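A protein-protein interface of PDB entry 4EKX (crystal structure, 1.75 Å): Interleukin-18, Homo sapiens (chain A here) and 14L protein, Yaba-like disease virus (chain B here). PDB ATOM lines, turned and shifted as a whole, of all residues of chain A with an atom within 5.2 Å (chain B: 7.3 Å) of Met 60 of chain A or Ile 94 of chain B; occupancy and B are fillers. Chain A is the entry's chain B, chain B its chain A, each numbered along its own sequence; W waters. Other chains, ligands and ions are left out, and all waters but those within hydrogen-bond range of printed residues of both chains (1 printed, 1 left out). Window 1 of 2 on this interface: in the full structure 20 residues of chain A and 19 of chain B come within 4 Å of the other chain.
The side-chain sulfur (SD) of Met 60 of chain A sits close to the backbone carbonyl oxygen (O) of Phe 32 of chain B (3.7 Å).
NE of Arg 5 of chain B is in salt-bridge range of OD2 of Asp 95 of chain B (2.7 Å). OD2 of Asp 95 of chain B lies within hydrogen-bond range of OG of Ser 27 of chain B (2.7 Å). O of Tyr 34 of chain B is in hydrogen-bond range of N of Ile 94 of chain B, at 2.8 Å. The backbone carbonyl oxygen (O) of Tyr 36 of chain B sits at hydrogen-bond distance from the backbone NH (N) of Val 92 of chain B, at 2.9 Å. The backbone NH (N) of Lys 97 of chain B sits at hydrogen-bond distance from the side-chain carboxylate (OD1) of Asp 95 of chain B, 2.9 Å away. O of Met 60 of chain A is in hydrogen-bond range of N of Gln 103 of chain A.
His 31 of chain B touches Met 51 of chain A (O to CE, 3.9 Å). Met 51 of chain A touches Phe 32 of chain B (SD to CD1, 3.8 Å). CG of Pro 57 of chain A touches OH of Tyr 36 of chain B (3.9 Å). Pro 57 of chain A touches Pro 99 of chain B (O to CG, 3.8 Å). Arg 58 of chain A touches Pro 99 of chain B (C to CG, 3.8 Å). Gly 59 of chain A touches Ile 94 of chain B. Pro 99 of chain B touches Gly 59 of chain A (CG to N, 3.6 Å). Met 60 of chain A touches Asp 95 of chain B. Tyr 34 of chain B touches Ala 61 of chain A (OH to O, 3.8 Å). Gln 103 of chain A touches Phe 32 of chain B (NE2 to CE2, 3.8 Å).
Of the printed residues of chain B, Gly 59 of chain A touches Ile 94 (3.7 Å) and Pro 99 (3.6 Å). Met 60 of chain A touches four residues of chain B. Of the printed residues of chain B, Ala 61 of chain A touches Tyr 34 (3.8 Å). Printed residues of chain B within 4 Å of Gln 103 of chain A: Phe 32 and Pro 96. Printed residues of chain A within 4 Å of Tyr 34 of chain B: Met 51, Met 60 and Ala 61. Of the printed residues of chain A, Ile 94 of chain B touches Gly 59 (3.7 Å) and Met 60 (3.4 Å). The nearest residue of chain B that does not touch Met 60 of chain A is Pro 96 of chain B (4.02 Å). The nearest printed residue of chain A that does not touch Phe 32 of chain B is Val 62 of chain A (5.7 Å).
Of the 10 printed residues of chain A, 7 touch a printed residue of chain B. Printed residues of chain A that touch a printed residue of chain B: Met 51, Pro 57, Arg 58, Gly 59, Met 60, Ala 61 and Gln 103. Printed residues of chain B that touch a printed residue of chain A: His 31, Phe 32, Tyr 34, Tyr 36, Val 92, Ile 94, Asp 95, Pro 96 and Pro 99. Hydrophobic or aromatic side chains of chain B that line the printed part of chain A: Phe 32, Tyr 34, Tyr 36, Val 92, Ile 94 and Pro 99. Among the printed residues, 16 pairs touch across the chains. Among the printed residues, no Asp or Glu carboxylate lies within 4 Å of a Lys or Arg side-chain nitrogen of the other chain.
Water W1 lies within hydrogen-bond range of O of Gly 59 of chain A, N of Ala 61 of chain A and OH of Tyr 34 of chain B.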
ATOM      1  N   MET A  51       4.023   8.318  -5.358  1.00  0.00           N
ATOM      2  CA  MET A  51       2.931   8.938  -6.092  1.00  0.00           C
ATOM      3  C   MET A  51       2.585   8.099  -7.333  1.00  0.00           C
ATOM      4  O   MET A  51       3.465   7.538  -7.968  1.00  0.00           O
ATOM      5  CB  MET A  51       3.338  10.353  -6.520  1.00  0.00           C
ATOM      6  CG  MET A  51       3.413  11.371  -5.386  1.00  0.00           C
ATOM      7  SD  MET A  51       4.244  12.904  -5.905  1.00  0.00           S
ATOM      8  CE  MET A  51       5.960  12.392  -5.969  1.00  0.00           C
ATOM      9  N   PRO A  57      -8.682  10.363 -12.662  1.00  0.00           N
ATOM     10  CA  PRO A  57      -8.159  11.370 -11.730  1.00  0.00           C
ATOM     11  C   PRO A  57      -9.132  11.883 -10.661  1.00  0.00           C
ATOM     12  O   PRO A  57     -10.105  12.576 -10.976  1.00  0.00           O
ATOM     13  CB  PRO A  57      -7.811  12.545 -12.648  1.00  0.00           C
ATOM     14  CG  PRO A  57      -7.546  11.907 -13.988  1.00  0.00           C
ATOM     15  CD  PRO A  57      -8.571  10.792 -14.063  1.00  0.00           C
ATOM     16  N   ARG A  58      -8.849  11.546  -9.404  1.00  0.00           N
ATOM     17  CA  ARG A  58      -9.706  11.901  -8.281  1.00  0.00           C
ATOM     18  C   ARG A  58      -8.965  12.709  -7.212  1.00  0.00           C
ATOM     19  O   ARG A  58      -9.575  13.378  -6.391  1.00  0.00           O
ATOM     20  CB  ARG A  58     -10.246  10.593  -7.694  1.00  0.00           C
ATOM     21  CG  ARG A  58     -11.347   9.958  -8.535  1.00  0.00           C
ATOM     22  CD  ARG A  58     -11.534   8.484  -8.193  1.00  0.00           C
ATOM     23  NE  ARG A  58     -10.404   7.690  -8.659  1.00  0.00           N
ATOM     24  CZ  ARG A  58     -10.220   6.405  -8.371  1.00  0.00           C
ATOM     25  NH1 ARG A  58     -11.083   5.765  -7.591  1.00  0.00           N
ATOM     26  NH2 ARG A  58      -9.161   5.773  -8.844  1.00  0.00           N
ATOM     27  N   GLY A  59      -7.642  12.645  -7.260  1.00  0.00           N
ATOM     28  CA  GLY A  59      -6.775  13.338  -6.328  1.00  0.00           C
ATOM     29  C   GLY A  59      -5.415  12.673  -6.422  1.00  0.00           C
ATOM     30  O   GLY A  59      -5.163  11.887  -7.347  1.00  0.00           O
ATOM     31  N   MET A  60      -4.529  12.968  -5.480  1.00  0.00           N
ATOM     32  CA  MET A  60      -3.192  12.388  -5.531  1.00  0.00           C
ATOM     33  C   MET A  60      -3.139  11.006  -4.885  1.00  0.00           C
ATOM     34  O   MET A  60      -3.194  10.869  -3.665  1.00  0.00           O
ATOM     35  CB  MET A  60      -2.167  13.328  -4.905  1.00  0.00           C
ATOM     36  CG  MET A  60      -0.737  12.866  -5.063  1.00  0.00           C
ATOM     37  SD  MET A  60       0.393  14.201  -4.614  1.00  0.00           S
ATOM     38  CE  MET A  60       0.144  14.246  -2.831  1.00  0.00           C
ATOM     39  N   ALA A  61      -3.034   9.984  -5.724  1.00  0.00           N
ATOM     40  CA  ALA A  61      -2.978   8.602  -5.247  1.00  0.00           C
ATOM     41  C   ALA A  61      -1.569   8.275  -4.763  1.00  0.00           C
ATOM     42  O   ALA A  61      -0.600   8.456  -5.509  1.00  0.00           O
ATOM     43  CB  ALA A  61      -3.394   7.635  -6.383  1.00  0.00           C
ATOM     44  N   VAL A  62      -1.456   7.784  -3.527  1.00  0.00           N
ATOM     45  CA  VAL A  62      -0.156   7.442  -2.959  1.00  0.00           C
ATOM     46  C   VAL A  62      -0.153   6.123  -2.190  1.00  0.00           C
ATOM     47  O   VAL A  62      -1.192   5.671  -1.710  1.00  0.00           O
ATOM     48  CB  VAL A  62       0.337   8.547  -1.991  1.00  0.00           C
ATOM     49  CG1 VAL A  62       0.364   9.882  -2.702  1.00  0.00           C
ATOM     50  CG2 VAL A  62      -0.552   8.611  -0.729  1.00  0.00           C
ATOM     51  N   PHE A 101      -3.961   5.403  -0.966  1.00  0.00           N
ATOM     52  CA  PHE A 101      -4.689   6.464  -0.283  1.00  0.00           C
ATOM     53  C   PHE A 101      -4.701   7.707  -1.151  1.00  0.00           C
ATOM     54  O   PHE A 101      -3.767   7.940  -1.920  1.00  0.00           O
ATOM     55  CB  PHE A 101      -4.015   6.785   1.052  1.00  0.00           C
ATOM     56  CG  PHE A 101      -4.005   5.625   2.009  1.00  0.00           C
ATOM     57  CD1 PHE A 101      -5.028   5.464   2.933  1.00  0.00           C
ATOM     58  CD2 PHE A 101      -2.995   4.674   1.955  1.00  0.00           C
ATOM     59  CE1 PHE A 101      -5.037   4.397   3.807  1.00  0.00           C
ATOM     60  CE2 PHE A 101      -3.000   3.592   2.830  1.00  0.00           C
ATOM     61  CZ  PHE A 101      -4.021   3.458   3.755  1.00  0.00           C
ATOM     62  N   PHE A 102      -5.750   8.516  -1.041  1.00  0.00           N
ATOM     63  CA  PHE A 102      -5.713   9.803  -1.721  1.00  0.00           C
ATOM     64  C   PHE A 102      -5.242  10.861  -0.742  1.00  0.00           C
ATOM     65  O   PHE A 102      -5.859  11.052   0.325  1.00  0.00           O
ATOM     66  CB  PHE A 102      -7.071  10.189  -2.284  1.00  0.00           C
ATOM     67  CG  PHE A 102      -7.556   9.266  -3.353  1.00  0.00           C
ATOM     68  CD1 PHE A 102      -6.937   9.229  -4.598  1.00  0.00           C
ATOM     69  CD2 PHE A 102      -8.648   8.450  -3.117  1.00  0.00           C
ATOM     70  CE1 PHE A 102      -7.397   8.359  -5.585  1.00  0.00           C
ATOM     71  CE2 PHE A 102      -9.112   7.585  -4.099  1.00  0.00           C
ATOM     72  CZ  PHE A 102      -8.480   7.549  -5.335  1.00  0.00           C
ATOM     73  N   GLN A 103      -4.148  11.524  -1.119  1.00  0.00           N
ATOM     74  CA  GLN A 103      -3.530  12.557  -0.292  1.00  0.00           C
ATOM     75  C   GLN A 103      -4.097  13.903  -0.698  1.00  0.00           C
ATOM     76  O   GLN A 103      -3.925  14.336  -1.830  1.00  0.00           O
ATOM     77  CB  GLN A 103      -2.012  12.546  -0.453  1.00  0.00           C
ATOM     78  CG  GLN A 103      -1.304  13.600   0.430  1.00  0.00           C
ATOM     79  CD  GLN A 103       0.199  13.551   0.326  1.00  0.00           C
ATOM     80  OE1 GLN A 103       0.780  12.489   0.110  1.00  0.00           O
ATOM     81  NE2 GLN A 103       0.847  14.711   0.488  1.00  0.00           N
ATOM     82  N   ARG B   5      -2.265  27.522  -9.676  1.00  0.00           N
ATOM     83  CA  ARG B   5      -2.256  26.162 -10.213  1.00  0.00           C
ATOM     84  C   ARG B   5      -2.836  26.129 -11.623  1.00  0.00           C
ATOM     85  O   ARG B   5      -3.893  26.705 -11.894  1.00  0.00           O
ATOM     86  CB  ARG B   5      -3.027  25.194  -9.319  1.00  0.00           C
ATOM     87  CG  ARG B   5      -2.373  24.957  -7.971  1.00  0.00           C
ATOM     88  CD  ARG B   5      -3.299  24.207  -7.039  1.00  0.00           C
ATOM     89  NE  ARG B   5      -3.580  22.834  -7.465  1.00  0.00           N
ATOM     90  CZ  ARG B   5      -4.752  22.423  -7.938  1.00  0.00           C
ATOM     91  NH1 ARG B   5      -5.756  23.280  -8.070  1.00  0.00           N
ATOM     92  NH2 ARG B   5      -4.927  21.148  -8.266  1.00  0.00           N
ATOM     93  N   VAL B   7      -2.530  23.876 -15.753  1.00  0.00           N
ATOM     94  CA  VAL B   7      -1.944  22.862 -16.612  1.00  0.00           C
ATOM     95  C   VAL B   7      -2.090  23.398 -18.031  1.00  0.00           C
ATOM     96  O   VAL B   7      -3.092  24.022 -18.368  1.00  0.00           O
ATOM     97  CB  VAL B   7      -2.615  21.475 -16.412  1.00  0.00           C
ATOM     98  CG1 VAL B   7      -4.110  21.531 -16.729  1.00  0.00           C
ATOM     99  CG2 VAL B   7      -1.912  20.403 -17.234  1.00  0.00           C
ATOM    100  N   SER B  27       2.273  24.251 -10.121  1.00  0.00           N
ATOM    101  CA  SER B  27       1.669  24.019  -8.808  1.00  0.00           C
ATOM    102  C   SER B  27       2.590  24.461  -7.689  1.00  0.00           C
ATOM    103  O   SER B  27       3.791  24.204  -7.723  1.00  0.00           O
ATOM    104  CB  SER B  27       1.307  22.541  -8.614  1.00  0.00           C
ATOM    105  OG  SER B  27       0.870  22.320  -7.270  1.00  0.00           O
ATOM    106  N   PHE B  29       2.450  23.276  -4.768  1.00  0.00           N
ATOM    107  CA  PHE B  29       2.797  22.081  -4.006  1.00  0.00           C
ATOM    108  C   PHE B  29       4.033  21.450  -4.629  1.00  0.00           C
ATOM    109  O   PHE B  29       3.935  20.504  -5.400  1.00  0.00           O
ATOM    110  CB  PHE B  29       1.631  21.084  -3.947  1.00  0.00           C
ATOM    111  CG  PHE B  29       0.423  21.609  -3.226  1.00  0.00           C
ATOM    112  CD1 PHE B  29       0.342  21.537  -1.845  1.00  0.00           C
ATOM    113  CD2 PHE B  29      -0.622  22.186  -3.925  1.00  0.00           C
ATOM    114  CE1 PHE B  29      -0.762  22.030  -1.173  1.00  0.00           C
ATOM    115  CE2 PHE B  29      -1.726  22.675  -3.269  1.00  0.00           C
ATOM    116  CZ  PHE B  29      -1.798  22.600  -1.881  1.00  0.00           C
ATOM    117  N   HIS B  31       6.685  19.501  -3.838  1.00  0.00           N
ATOM    118  CA  HIS B  31       7.146  18.117  -3.736  1.00  0.00           C
ATOM    119  C   HIS B  31       6.104  17.119  -4.227  1.00  0.00           C
ATOM    120  O   HIS B  31       6.394  15.935  -4.426  1.00  0.00           O
ATOM    121  CB  HIS B  31       7.540  17.776  -2.301  1.00  0.00           C
ATOM    122  CG  HIS B  31       8.721  18.546  -1.797  1.00  0.00           C
ATOM    123  ND1 HIS B  31       9.998  18.344  -2.277  1.00  0.00           N
ATOM    124  CD2 HIS B  31       8.821  19.509  -0.854  1.00  0.00           C
ATOM    125  CE1 HIS B  31      10.834  19.155  -1.652  1.00  0.00           C
ATOM    126  NE2 HIS B  31      10.146  19.871  -0.783  1.00  0.00           N
ATOM    127  N   PHE B  32       4.886  17.597  -4.422  1.00  0.00           N
ATOM    128  CA  PHE B  32       3.779  16.692  -4.686  1.00  0.00           C
ATOM    129  C   PHE B  32       2.938  17.202  -5.841  1.00  0.00           C
ATOM    130  O   PHE B  32       1.761  17.507  -5.671  1.00  0.00           O
ATOM    131  CB  PHE B  32       2.901  16.547  -3.441  1.00  0.00           C
ATOM    132  CG  PHE B  32       3.559  15.797  -2.312  1.00  0.00           C
ATOM    133  CD1 PHE B  32       3.849  14.443  -2.439  1.00  0.00           C
ATOM    134  CD2 PHE B  32       3.869  16.436  -1.122  1.00  0.00           C
ATOM    135  CE1 PHE B  32       4.451  13.745  -1.404  1.00  0.00           C
ATOM    136  CE2 PHE B  32       4.467  15.745  -0.077  1.00  0.00           C
ATOM    137  CZ  PHE B  32       4.764  14.398  -0.221  1.00  0.00           C
ATOM    138  N   SER B  33       3.537  17.314  -7.020  1.00  0.00           N
ATOM    139  CA  SER B  33       2.746  17.664  -8.189  1.00  0.00           C
ATOM    140  C   SER B  33       3.323  16.992  -9.407  1.00  0.00           C
ATOM    141  O   SER B  33       4.531  16.842  -9.534  1.00  0.00           O
ATOM    142  CB  SER B  33       2.694  19.177  -8.400  1.00  0.00           C
ATOM    143  OG  SER B  33       3.998  19.705  -8.491  1.00  0.00           O
ATOM    144  N   TYR B  34       2.445  16.559 -10.290  1.00  0.00           N
ATOM    145  CA  TYR B  34       2.907  15.893 -11.489  1.00  0.00           C
ATOM    146  C   TYR B  34       1.851  15.991 -12.568  1.00  0.00           C
ATOM    147  O   TYR B  34       0.689  16.235 -12.270  1.00  0.00           O
ATOM    148  CB  TYR B  34       3.302  14.433 -11.189  1.00  0.00           C
ATOM    149  CG  TYR B  34       2.348  13.616 -10.336  1.00  0.00           C
ATOM    150  CD1 TYR B  34       2.325  13.749  -8.949  1.00  0.00           C
ATOM    151  CD2 TYR B  34       1.513  12.646 -10.914  1.00  0.00           C
ATOM    152  CE1 TYR B  34       1.476  12.979  -8.173  1.00  0.00           C
ATOM    153  CE2 TYR B  34       0.665  11.872 -10.141  1.00  0.00           C
ATOM    154  CZ  TYR B  34       0.645  12.042  -8.774  1.00  0.00           C
ATOM    155  OH  TYR B  34      -0.197  11.267  -8.008  1.00  0.00           O
ATOM    156  N   VAL B  35       2.268  15.819 -13.820  1.00  0.00           N
ATOM    157  CA  VAL B  35       1.335  15.784 -14.938  1.00  0.00           C
ATOM    158  C   VAL B  35       1.518  14.507 -15.756  1.00  0.00           C
ATOM    159  O   VAL B  35       2.584  13.894 -15.761  1.00  0.00           O
ATOM    160  CB  VAL B  35       1.476  17.013 -15.865  1.00  0.00           C
ATOM    161  CG1 VAL B  35       1.101  18.306 -15.117  1.00  0.00           C
ATOM    162  CG2 VAL B  35       2.896  17.104 -16.434  1.00  0.00           C
ATOM    163  N   TYR B  36       0.451  14.090 -16.424  1.00  0.00           N
ATOM    164  CA  TYR B  36       0.541  12.956 -17.351  1.00  0.00           C
ATOM    165  C   TYR B  36      -0.652  12.958 -18.269  1.00  0.00           C
ATOM    166  O   TYR B  36      -1.618  13.701 -18.061  1.00  0.00           O
ATOM    167  CB  TYR B  36       0.587  11.628 -16.603  1.00  0.00           C
ATOM    168  CG  TYR B  36      -0.614  11.407 -15.717  1.00  0.00           C
ATOM    169  CD1 TYR B  36      -0.659  11.944 -14.421  1.00  0.00           C
ATOM    170  CD2 TYR B  36      -1.708  10.661 -16.164  1.00  0.00           C
ATOM    171  CE1 TYR B  36      -1.762  11.739 -13.599  1.00  0.00           C
ATOM    172  CE2 TYR B  36      -2.815  10.462 -15.347  1.00  0.00           C
ATOM    173  CZ  TYR B  36      -2.836  11.003 -14.064  1.00  0.00           C
ATOM    174  OH  TYR B  36      -3.921  10.814 -13.231  1.00  0.00           O
ATOM    175  N   PRO B  71       6.053  20.501 -13.269  1.00  0.00           N
ATOM    176  CA  PRO B  71       6.042  19.151 -13.832  1.00  0.00           C
ATOM    177  C   PRO B  71       5.780  19.183 -15.338  1.00  0.00           C
ATOM    178  O   PRO B  71       5.077  20.067 -15.829  1.00  0.00           O
ATOM    179  CB  PRO B  71       4.870  18.474 -13.106  1.00  0.00           C
ATOM    180  CG  PRO B  71       4.028  19.596 -12.589  1.00  0.00           C
ATOM    181  CD  PRO B  71       4.980  20.715 -12.283  1.00  0.00           C
ATOM    182  N   VAL B  92      -3.352  15.935 -17.381  1.00  0.00           N
ATOM    183  CA  VAL B  92      -3.897  16.068 -16.039  1.00  0.00           C
ATOM    184  C   VAL B  92      -2.809  16.546 -15.099  1.00  0.00           C
ATOM    185  O   VAL B  92      -1.698  16.028 -15.123  1.00  0.00           O
ATOM    186  CB  VAL B  92      -4.425  14.723 -15.513  1.00  0.00           C
ATOM    187  CG1 VAL B  92      -5.121  14.904 -14.141  1.00  0.00           C
ATOM    188  CG2 VAL B  92      -5.363  14.083 -16.532  1.00  0.00           C
ATOM    189  N   LEU B  93      -3.140  17.535 -14.276  1.00  0.00           N
ATOM    190  CA  LEU B  93      -2.282  17.917 -13.162  1.00  0.00           C
ATOM    191  C   LEU B  93      -2.801  17.276 -11.886  1.00  0.00           C
ATOM    192  O   LEU B  93      -3.962  17.449 -11.523  1.00  0.00           O
ATOM    193  CB  LEU B  93      -2.248  19.441 -12.990  1.00  0.00           C
ATOM    194  CG  LEU B  93      -1.651  19.908 -11.652  1.00  0.00           C
ATOM    195  CD1 LEU B  93      -0.154  19.638 -11.601  1.00  0.00           C
ATOM    196  CD2 LEU B  93      -1.937  21.391 -11.404  1.00  0.00           C
ATOM    197  N   ILE B  94      -1.935  16.524 -11.219  1.00  0.00           N
ATOM    198  CA  ILE B  94      -2.259  15.940  -9.922  1.00  0.00           C
ATOM    199  C   ILE B  94      -1.411  16.598  -8.850  1.00  0.00           C
ATOM    200  O   ILE B  94      -0.213  16.746  -9.016  1.00  0.00           O
ATOM    201  CB  ILE B  94      -1.998  14.411  -9.903  1.00  0.00           C
ATOM    202  CG1 ILE B  94      -2.878  13.709 -10.936  1.00  0.00           C
ATOM    203  CG2 ILE B  94      -2.272  13.841  -8.511  1.00  0.00           C
ATOM    204  CD1 ILE B  94      -4.360  13.886 -10.701  1.00  0.00           C
ATOM    205  N   ASP B  95      -2.058  17.004  -7.759  1.00  0.00           N
ATOM    206  CA  ASP B  95      -1.375  17.500  -6.559  1.00  0.00           C
ATOM    207  C   ASP B  95      -2.371  17.396  -5.392  1.00  0.00           C
ATOM    208  O   ASP B  95      -3.451  16.847  -5.576  1.00  0.00           O
ATOM    209  CB  ASP B  95      -0.817  18.928  -6.748  1.00  0.00           C
ATOM    210  CG  ASP B  95      -1.893  19.985  -6.962  1.00  0.00           C
ATOM    211  OD1 ASP B  95      -3.089  19.695  -6.776  1.00  0.00           O
ATOM    212  OD2 ASP B  95      -1.525  21.135  -7.309  1.00  0.00           O
ATOM    213  N   PRO B  96      -2.030  17.907  -4.217  1.00  0.00           N
ATOM    214  CA  PRO B  96      -2.930  17.786  -3.065  1.00  0.00           C
ATOM    215  C   PRO B  96      -4.307  18.441  -3.213  1.00  0.00           C
ATOM    216  O   PRO B  96      -5.136  18.331  -2.318  1.00  0.00           O
ATOM    217  CB  PRO B  96      -2.129  18.440  -1.949  1.00  0.00           C
ATOM    218  CG  PRO B  96      -0.721  18.141  -2.317  1.00  0.00           C
ATOM    219  CD  PRO B  96      -0.654  18.167  -3.820  1.00  0.00           C
ATOM    220  N   LYS B  97      -4.551  19.115  -4.331  1.00  0.00           N
ATOM    221  CA  LYS B  97      -5.864  19.691  -4.591  1.00  0.00           C
ATOM    222  C   LYS B  97      -6.570  18.956  -5.739  1.00  0.00           C
ATOM    223  O   LYS B  97      -6.006  18.049  -6.328  1.00  0.00           O
ATOM    224  CB  LYS B  97      -5.759  21.194  -4.858  1.00  0.00           C
ATOM    225  CG  LYS B  97      -5.278  21.997  -3.658  1.00  0.00           C
ATOM    226  CD  LYS B  97      -5.184  23.485  -3.952  1.00  0.00           C
ATOM    227  CE  LYS B  97      -4.656  24.255  -2.755  1.00  0.00           C
ATOM    228  N   ASP B  98      -7.807  19.336  -6.032  1.00  0.00           N
ATOM    229  CA  ASP B  98      -8.594  18.685  -7.069  1.00  0.00           C
ATOM    230  C   ASP B  98      -7.843  18.712  -8.389  1.00  0.00           C
ATOM    231  O   ASP B  98      -7.255  19.721  -8.739  1.00  0.00           O
ATOM    232  CB  ASP B  98      -9.948  19.372  -7.228  1.00  0.00           C
ATOM    233  CG  ASP B  98     -10.897  19.072  -6.080  1.00  0.00           C
ATOM    234  OD1 ASP B  98     -10.783  17.993  -5.471  1.00  0.00           O
ATOM    235  OD2 ASP B  98     -11.757  19.917  -5.790  1.00  0.00           O
ATOM    236  N   PRO B  99      -7.856  17.599  -9.114  1.00  0.00           N
ATOM    237  CA  PRO B  99      -7.088  17.525 -10.367  1.00  0.00           C
ATOM    238  C   PRO B  99      -7.517  18.583 -11.391  1.00  0.00           C
ATOM    239  O   PRO B  99      -8.695  18.958 -11.448  1.00  0.00           O
ATOM    240  CB  PRO B  99      -7.401  16.112 -10.882  1.00  0.00           C
ATOM    241  CG  PRO B  99      -7.855  15.350  -9.654  1.00  0.00           C
ATOM    242  CD  PRO B  99      -8.585  16.352  -8.830  1.00  0.00           C
ATOM    243  N   LEU B 100      -6.556  19.077 -12.161  1.00  0.00           N
ATOM    244  CA  LEU B 100      -6.824  20.033 -13.235  1.00  0.00           C
ATOM    245  C   LEU B 100      -6.554  19.349 -14.562  1.00  0.00           C
ATOM    246  O   LEU B 100      -5.616  18.556 -14.674  1.00  0.00           O
ATOM    247  CB  LEU B 100      -5.934  21.277 -13.116  1.00  0.00           C
ATOM    248  CG  LEU B 100      -6.174  22.220 -11.938  1.00  0.00           C
ATOM    249  CD1 LEU B 100      -5.305  23.468 -12.094  1.00  0.00           C
ATOM    250  CD2 LEU B 100      -7.646  22.592 -11.841  1.00  0.00           C
HETATM  251  O   HOH W   1      -3.267  10.125  -8.705  1.00  0.00           O
